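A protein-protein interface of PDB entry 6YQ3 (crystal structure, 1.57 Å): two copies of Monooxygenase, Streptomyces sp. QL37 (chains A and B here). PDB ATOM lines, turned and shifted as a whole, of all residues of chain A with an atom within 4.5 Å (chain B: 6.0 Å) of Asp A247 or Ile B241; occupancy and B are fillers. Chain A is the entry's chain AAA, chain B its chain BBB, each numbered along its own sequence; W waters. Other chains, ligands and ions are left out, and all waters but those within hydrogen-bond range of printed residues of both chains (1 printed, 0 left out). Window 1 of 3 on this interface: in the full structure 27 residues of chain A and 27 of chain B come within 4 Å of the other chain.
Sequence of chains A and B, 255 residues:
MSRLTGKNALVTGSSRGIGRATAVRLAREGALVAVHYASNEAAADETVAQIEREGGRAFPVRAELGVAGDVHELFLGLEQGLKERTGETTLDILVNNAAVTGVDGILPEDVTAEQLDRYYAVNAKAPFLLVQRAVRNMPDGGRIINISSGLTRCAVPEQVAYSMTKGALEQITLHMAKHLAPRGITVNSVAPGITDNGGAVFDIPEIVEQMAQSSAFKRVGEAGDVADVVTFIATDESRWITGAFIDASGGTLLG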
ATOM      1  N   ALA A 191      10.120  32.121  18.821  1.00  0.00           N
ATOM      2  CA  ALA A 191       8.807  32.617  18.399  1.00  0.00           C
ATOM      3  C   ALA A 191       7.700  31.727  18.906  1.00  0.00           C
ATOM      4  O   ALA A 191       7.474  30.672  18.324  1.00  0.00           O
ATOM      5  CB  ALA A 191       8.751  32.665  16.911  1.00  0.00           C
ATOM      6  N   VAL A 229      12.128  25.567  25.503  1.00  0.00           N
ATOM      7  CA  VAL A 229      13.006  25.900  24.336  1.00  0.00           C
ATOM      8  C   VAL A 229      13.949  27.029  24.711  1.00  0.00           C
ATOM      9  O   VAL A 229      15.174  26.946  24.406  1.00  0.00           O
ATOM     10  CB  VAL A 229      12.185  26.289  23.092  1.00  0.00           C
ATOM     11  CG1 VAL A 229      13.043  26.729  21.943  1.00  0.00           C
ATOM     12  CG2 VAL A 229      11.275  25.162  22.681  1.00  0.00           C
ATOM     13  N   PHE A 245      15.925  32.055  13.915  1.00  0.00           N
ATOM     14  CA  PHE A 245      14.502  32.043  14.235  1.00  0.00           C
ATOM     15  C   PHE A 245      14.129  30.647  14.687  1.00  0.00           C
ATOM     16  O   PHE A 245      14.210  29.733  13.852  1.00  0.00           O
ATOM     17  CB  PHE A 245      13.722  32.464  12.994  1.00  0.00           C
ATOM     18  CG  PHE A 245      12.235  32.480  13.173  1.00  0.00           C
ATOM     19  CD1 PHE A 245      11.586  33.614  13.682  1.00  0.00           C
ATOM     20  CD2 PHE A 245      11.456  31.348  12.892  1.00  0.00           C
ATOM     21  CE1 PHE A 245      10.184  33.634  13.830  1.00  0.00           C
ATOM     22  CE2 PHE A 245      10.068  31.380  13.054  1.00  0.00           C
ATOM     23  CZ  PHE A 245       9.435  32.528  13.487  1.00  0.00           C
ATOM     24  N   ILE A 246      13.800  30.474  15.951  1.00  0.00           N
ATOM     25  CA  ILE A 246      13.489  29.155  16.551  1.00  0.00           C
ATOM     26  C   ILE A 246      11.979  29.162  16.738  1.00  0.00           C
ATOM     27  O   ILE A 246      11.447  29.912  17.569  1.00  0.00           O
ATOM     28  CB  ILE A 246      14.250  28.928  17.872  1.00  0.00           C
ATOM     29  CG1 ILE A 246      15.762  29.056  17.703  1.00  0.00           C
ATOM     30  CG2 ILE A 246      13.867  27.567  18.388  1.00  0.00           C
ATOM     31  CD1 ILE A 246      16.379  28.065  16.783  1.00  0.00           C
ATOM     32  N   ASP A 247      11.314  28.315  15.981  1.00  0.00           N
ATOM     33  CA  ASP A 247       9.850  28.218  15.993  1.00  0.00           C
ATOM     34  C   ASP A 247       9.433  27.389  17.206  1.00  0.00           C
ATOM     35  O   ASP A 247       9.708  26.193  17.212  1.00  0.00           O
ATOM     36  CB  ASP A 247       9.375  27.625  14.684  1.00  0.00           C
ATOM     37  CG  ASP A 247       7.880  27.569  14.556  1.00  0.00           C
ATOM     38  OD1 ASP A 247       7.161  27.307  15.539  1.00  0.00           O
ATOM     39  OD2 ASP A 247       7.455  27.718  13.426  1.00  0.00           O
ATOM     40  N   ALA A 248       8.833  28.035  18.196  1.00  0.00           N
ATOM     41  CA  ALA A 248       8.297  27.356  19.385  1.00  0.00           C
ATOM     42  C   ALA A 248       6.794  27.613  19.424  1.00  0.00           C
ATOM     43  O   ALA A 248       6.238  28.103  20.445  1.00  0.00           O
ATOM     44  CB  ALA A 248       9.021  27.840  20.631  1.00  0.00           C
ATOM     45  N   SER A 249       6.117  27.307  18.323  1.00  0.00           N
ATOM     46  CA  SER A 249       4.683  27.635  18.138  1.00  0.00           C
ATOM     47  C   SER A 249       3.812  26.385  18.056  1.00  0.00           C
ATOM     48  O   SER A 249       2.589  26.565  17.797  1.00  0.00           O
ATOM     49  CB  SER A 249       4.453  28.505  16.921  1.00  0.00           C
ATOM     50  OG  SER A 249       4.597  27.747  15.743  1.00  0.00           O
ATOM     51  N   GLY A 250       4.367  25.171  18.286  1.00  0.00           N
ATOM     52  CA  GLY A 250       3.523  23.979  18.116  1.00  0.00           C
ATOM     53  C   GLY A 250       3.003  23.880  16.697  1.00  0.00           C
ATOM     54  O   GLY A 250       1.805  23.514  16.497  1.00  0.00           O
ATOM     55  N   LEU A 253       2.900  27.717  12.147  1.00  0.00           N
ATOM     56  CA  LEU A 253       3.195  28.253  10.780  1.00  0.00           C
ATOM     57  C   LEU A 253       2.945  27.189   9.693  1.00  0.00           C
ATOM     58  O   LEU A 253       3.094  27.552   8.537  1.00  0.00           O
ATOM     59  CB  LEU A 253       4.622  28.774  10.801  1.00  0.00           C
ATOM     60  CG  LEU A 253       4.874  29.822  11.886  1.00  0.00           C
ATOM     61  CD1 LEU A 253       6.283  30.374  11.751  1.00  0.00           C
ATOM     62  CD2 LEU A 253       3.857  30.939  11.765  1.00  0.00           C
ATOM     63  N   THR B 186       7.042  14.828  16.028  1.00  0.00           N
ATOM     64  CA  THR B 186       7.584  16.085  15.473  1.00  0.00           C
ATOM     65  C   THR B 186       8.506  15.738  14.306  1.00  0.00           C
ATOM     66  O   THR B 186       9.117  14.679  14.316  1.00  0.00           O
ATOM     67  CB  THR B 186       8.256  16.983  16.499  1.00  0.00           C
ATOM     68  OG1 THR B 186       9.472  16.361  16.911  1.00  0.00           O
ATOM     69  CG2 THR B 186       7.291  17.288  17.643  1.00  0.00           C
ATOM     70  N   VAL B 187       8.611  16.654  13.382  1.00  0.00           N
ATOM     71  CA  VAL B 187       9.495  16.497  12.191  1.00  0.00           C
ATOM     72  C   VAL B 187      10.207  17.813  11.988  1.00  0.00           C
ATOM     73  O   VAL B 187       9.533  18.819  11.749  1.00  0.00           O
ATOM     74  CB  VAL B 187       8.735  16.101  10.917  1.00  0.00           C
ATOM     75  CG1 VAL B 187       9.718  15.734   9.811  1.00  0.00           C
ATOM     76  CG2 VAL B 187       7.751  14.969  11.165  1.00  0.00           C
ATOM     77  N   ASN B 188      11.534  17.786  12.012  1.00  0.00           N
ATOM     78  CA  ASN B 188      12.314  19.048  11.967  1.00  0.00           C
ATOM     79  C   ASN B 188      13.559  18.850  11.129  1.00  0.00           C
ATOM     80  O   ASN B 188      14.005  17.680  11.031  1.00  0.00           O
ATOM     81  CB  ASN B 188      12.750  19.498  13.355  1.00  0.00           C
ATOM     82  CG  ASN B 188      11.582  20.002  14.198  1.00  0.00           C
ATOM     83  OD1 ASN B 188      10.914  20.972  13.809  1.00  0.00           O
ATOM     84  ND2 ASN B 188      11.266  19.269  15.275  1.00  0.00           N
ATOM     85  N   PHE B 232      19.181  17.538  21.374  1.00  0.00           N
ATOM     86  CA  PHE B 232      18.110  18.320  22.020  1.00  0.00           C
ATOM     87  C   PHE B 232      16.770  18.065  21.296  1.00  0.00           C
ATOM     88  O   PHE B 232      15.733  17.848  21.964  1.00  0.00           O
ATOM     89  CB  PHE B 232      18.440  19.802  22.042  1.00  0.00           C
ATOM     90  CG  PHE B 232      17.208  20.600  22.365  1.00  0.00           C
ATOM     91  CD1 PHE B 232      16.678  20.581  23.644  1.00  0.00           C
ATOM     92  CD2 PHE B 232      16.565  21.333  21.361  1.00  0.00           C
ATOM     93  CE1 PHE B 232      15.475  21.249  23.903  1.00  0.00           C
ATOM     94  CE2 PHE B 232      15.389  22.006  21.649  1.00  0.00           C
ATOM     95  CZ  PHE B 232      14.853  21.943  22.895  1.00  0.00           C
ATOM     96  N   ILE B 233      16.778  18.149  19.941  1.00  0.00           N
ATOM     97  CA  ILE B 233      15.504  17.914  19.212  1.00  0.00           C
ATOM     98  C   ILE B 233      14.941  16.540  19.504  1.00  0.00           C
ATOM     99  O   ILE B 233      13.716  16.428  19.628  1.00  0.00           O
ATOM    100  CB  ILE B 233      15.670  18.201  17.702  1.00  0.00           C
ATOM    101  CG1 ILE B 233      16.141  19.629  17.456  1.00  0.00           C
ATOM    102  CG2 ILE B 233      14.373  17.826  16.958  1.00  0.00           C
ATOM    103  CD1 ILE B 233      15.120  20.715  17.739  1.00  0.00           C
ATOM    104  N   GLU B 237      11.827  17.990  25.600  1.00  0.00           N
ATOM    105  CA  GLU B 237      11.757  19.453  25.792  1.00  0.00           C
ATOM    106  C   GLU B 237      11.631  20.179  24.449  1.00  0.00           C
ATOM    107  O   GLU B 237      11.378  21.370  24.474  1.00  0.00           O
ATOM    108  CB  GLU B 237      12.955  19.976  26.601  1.00  0.00           C
ATOM    109  CG  GLU B 237      12.814  19.682  28.098  1.00  0.00           C
ATOM    110  CD  GLU B 237      12.941  18.225  28.501  1.00  0.00           C
ATOM    111  OE1 GLU B 237      13.693  17.487  27.878  1.00  0.00           O
ATOM    112  OE2 GLU B 237      12.138  17.804  29.392  1.00  0.00           O
ATOM    113  N   SER B 238      11.755  19.498  23.322  1.00  0.00           N
ATOM    114  CA  SER B 238      11.597  20.106  21.986  1.00  0.00           C
ATOM    115  C   SER B 238      10.152  19.917  21.488  1.00  0.00           C
ATOM    116  O   SER B 238       9.939  20.250  20.321  1.00  0.00           O
ATOM    117  CB  SER B 238      12.524  19.518  21.007  1.00  0.00           C
ATOM    118  OG  SER B 238      12.064  18.204  20.658  1.00  0.00           O
ATOM    119  N   ARG B 239       9.222  19.428  22.302  1.00  0.00           N
ATOM    120  CA  ARG B 239       7.893  19.001  21.840  1.00  0.00           C
ATOM    121  C   ARG B 239       7.163  20.099  21.077  1.00  0.00           C
ATOM    122  O   ARG B 239       6.292  19.729  20.304  1.00  0.00           O
ATOM    123  CB  ARG B 239       7.029  18.530  22.993  1.00  0.00           C
ATOM    124  CG  ARG B 239       6.581  19.647  23.924  1.00  0.00           C
ATOM    125  CD  ARG B 239       5.960  19.113  25.213  1.00  0.00           C
ATOM    126  NE  ARG B 239       7.001  18.750  26.152  1.00  0.00           N
ATOM    127  CZ  ARG B 239       7.705  19.639  26.881  1.00  0.00           C
ATOM    128  NH1 ARG B 239       8.675  19.246  27.675  1.00  0.00           N
ATOM    129  NH2 ARG B 239       7.370  20.913  26.859  1.00  0.00           N
ATOM    130  N   TRP B 240       7.414  21.368  21.381  1.00  0.00           N
ATOM    131  CA  TRP B 240       6.609  22.438  20.762  1.00  0.00           C
ATOM    132  C   TRP B 240       7.311  22.961  19.502  1.00  0.00           C
ATOM    133  O   TRP B 240       6.844  23.955  18.922  1.00  0.00           O
ATOM    134  CB  TRP B 240       6.382  23.515  21.849  1.00  0.00           C
ATOM    135  CG  TRP B 240       5.103  24.252  21.659  1.00  0.00           C
ATOM    136  CD1 TRP B 240       4.958  25.607  21.645  1.00  0.00           C
ATOM    137  CD2 TRP B 240       3.800  23.689  21.497  1.00  0.00           C
ATOM    138  NE1 TRP B 240       3.634  25.930  21.544  1.00  0.00           N
ATOM    139  CE2 TRP B 240       2.917  24.791  21.388  1.00  0.00           C
ATOM    140  CE3 TRP B 240       3.281  22.395  21.429  1.00  0.00           C
ATOM    141  CZ2 TRP B 240       1.561  24.615  21.201  1.00  0.00           C
ATOM    142  CZ3 TRP B 240       1.913  22.223  21.243  1.00  0.00           C
ATOM    143  CH2 TRP B 240       1.087  23.329  21.094  1.00  0.00           C
ATOM    144  N   ILE B 241       8.356  22.301  19.037  1.00  0.00           N
ATOM    145  CA  ILE B 241       9.066  22.597  17.782  1.00  0.00           C
ATOM    146  C   ILE B 241       8.689  21.506  16.802  1.00  0.00           C
ATOM    147  O   ILE B 241       9.093  20.383  16.969  1.00  0.00           O
ATOM    148  CB  ILE B 241      10.569  22.653  18.019  1.00  0.00           C
ATOM    149  CG1 ILE B 241      11.004  23.630  19.131  1.00  0.00           C
ATOM    150  CG2 ILE B 241      11.261  22.978  16.680  1.00  0.00           C
ATOM    151  CD1 ILE B 241      12.558  23.628  19.299  1.00  0.00           C
ATOM    152  N   THR B 242       8.025  21.889  15.722  1.00  0.00           N
ATOM    153  CA  THR B 242       7.770  20.976  14.596  1.00  0.00           C
ATOM    154  C   THR B 242       7.723  21.768  13.301  1.00  0.00           C
ATOM    155  O   THR B 242       7.337  22.947  13.304  1.00  0.00           O
ATOM    156  CB  THR B 242       6.527  20.146  14.822  1.00  0.00           C
ATOM    157  OG1 THR B 242       6.642  19.006  13.949  1.00  0.00           O
ATOM    158  CG2 THR B 242       5.229  20.865  14.579  1.00  0.00           C
ATOM    159  N   GLY B 243       8.041  21.075  12.213  1.00  0.00           N
ATOM    160  CA  GLY B 243       8.082  21.710  10.885  1.00  0.00           C
ATOM    161  C   GLY B 243       9.143  22.763  10.722  1.00  0.00           C
ATOM    162  O   GLY B 243       9.061  23.551   9.752  1.00  0.00           O
ATOM    163  N   ALA B 244      10.181  22.808  11.560  1.00  0.00           N
ATOM    164  CA  ALA B 244      11.100  23.937  11.676  1.00  0.00           C
ATOM    165  C   ALA B 244      12.379  23.674  10.909  1.00  0.00           C
ATOM    166  O   ALA B 244      12.798  22.520  10.824  1.00  0.00           O
ATOM    167  CB  ALA B 244      11.413  24.208  13.133  1.00  0.00           C
ATOM    168  N   ILE B 246      16.084  24.430  11.783  1.00  0.00           N
ATOM    169  CA  ILE B 246      16.938  24.756  12.933  1.00  0.00           C
ATOM    170  C   ILE B 246      18.342  24.948  12.395  1.00  0.00           C
ATOM    171  O   ILE B 246      18.961  23.977  11.897  1.00  0.00           O
ATOM    172  CB  ILE B 246      16.868  23.650  14.003  1.00  0.00           C
ATOM    173  CG1 ILE B 246      15.458  23.323  14.490  1.00  0.00           C
ATOM    174  CG2 ILE B 246      17.793  23.961  15.165  1.00  0.00           C
ATOM    175  CD1 ILE B 246      14.753  24.459  15.113  1.00  0.00           C
HETATM  176  O   HOH W   1       6.757  24.600  16.073  1.00  0.00           O
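The backbone NH (N) of Ser A249 sits at hydrogen-bond distance from the backbone carbonyl oxygen (O) of Trp B240, 3.5 Å away.
The backbone NH of Gly A250 lies within hydrogen-bond range of the backbone carbonyl oxygen of Trp B240, at 2.8 Å.
The backbone carbonyl oxygen (O) of Ala A191 lies within hydrogen-bond range of the backbone NH (N) of Ala A248 (3.0 Å).
OD1 of Asp A247 is in hydrogen-bond range of OG of Ser A249 (2.6 Å).
ND2 of Asn B188 lies within hydrogen-bond range of O of Ile B241, at 3.0 Å.
Ile B241 touches Val A229 (CG1 to CG2, 3.9 Å).
Ile B241 touches Asp A247 (CG1 to O, 3.5 Å).
Trp B240 touches Ala A248 (CD1 to O, 3.1 Å).
Of the 9 printed residues of chain A, 5 touch a printed residue of chain B.
Printed residues of chain A that touch a printed residue of chain B: Val A229, Asp A247, Ala A248, Ser A249 and Gly A250.
Hydrophobic or aromatic side chains of chain A that line the printed part of chain B: Val A229.
Of the 14 printed residues of chain B, 2 touch a printed residue of chain A.
Hydrophobic or aromatic side chains of chain B that line the printed part of chain A: Trp B240 and Ile B241.
Along chain B the printed residues that touch a printed residue of chain A span positions 240 to 241.
Among the printed residues, no Asp or Glu carboxylate lies within 4 Å of a Lys or Arg side-chain nitrogen of the other chain.
1 position is printed for both chains.
Of the 5 pairs that touch across the chains among the printed residues, none has its exchanged pair printed and touching as well.
Water W1 lies within hydrogen-bond range of OD1 of Asp A247 (2.8 Å), O of Trp B240 (2.9 Å), N of Thr B242 (3.0 Å) and N of Gly A250 (3.3 Å).
Of the printed residues of chain B, Asp A247 touches Ile B241.
Of the printed residues of chain B, Ala A248 touches Trp B240 (3.1 Å).
Of the printed residues of chain B, Ser A249 touches Trp B240 (3.5 Å).
Of the printed residues of chain B, Gly A250 touches Trp B240 (2.8 Å).
Leu A253 touches none of the printed residues of chain B.
Of the printed residues of chain A, Trp B240 touches Ala A248 (3.1 Å), Ser A249 (3.5 Å) and Gly A250 (2.8 Å).
Printed residues of chain A within 4 Å of Ile B241: Val A229 (3.9 Å) and Asp A247 (3.5 Å).
The nearest printed residue of chain B that does not touch Asp A247 is Trp B240 (4.02 Å).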
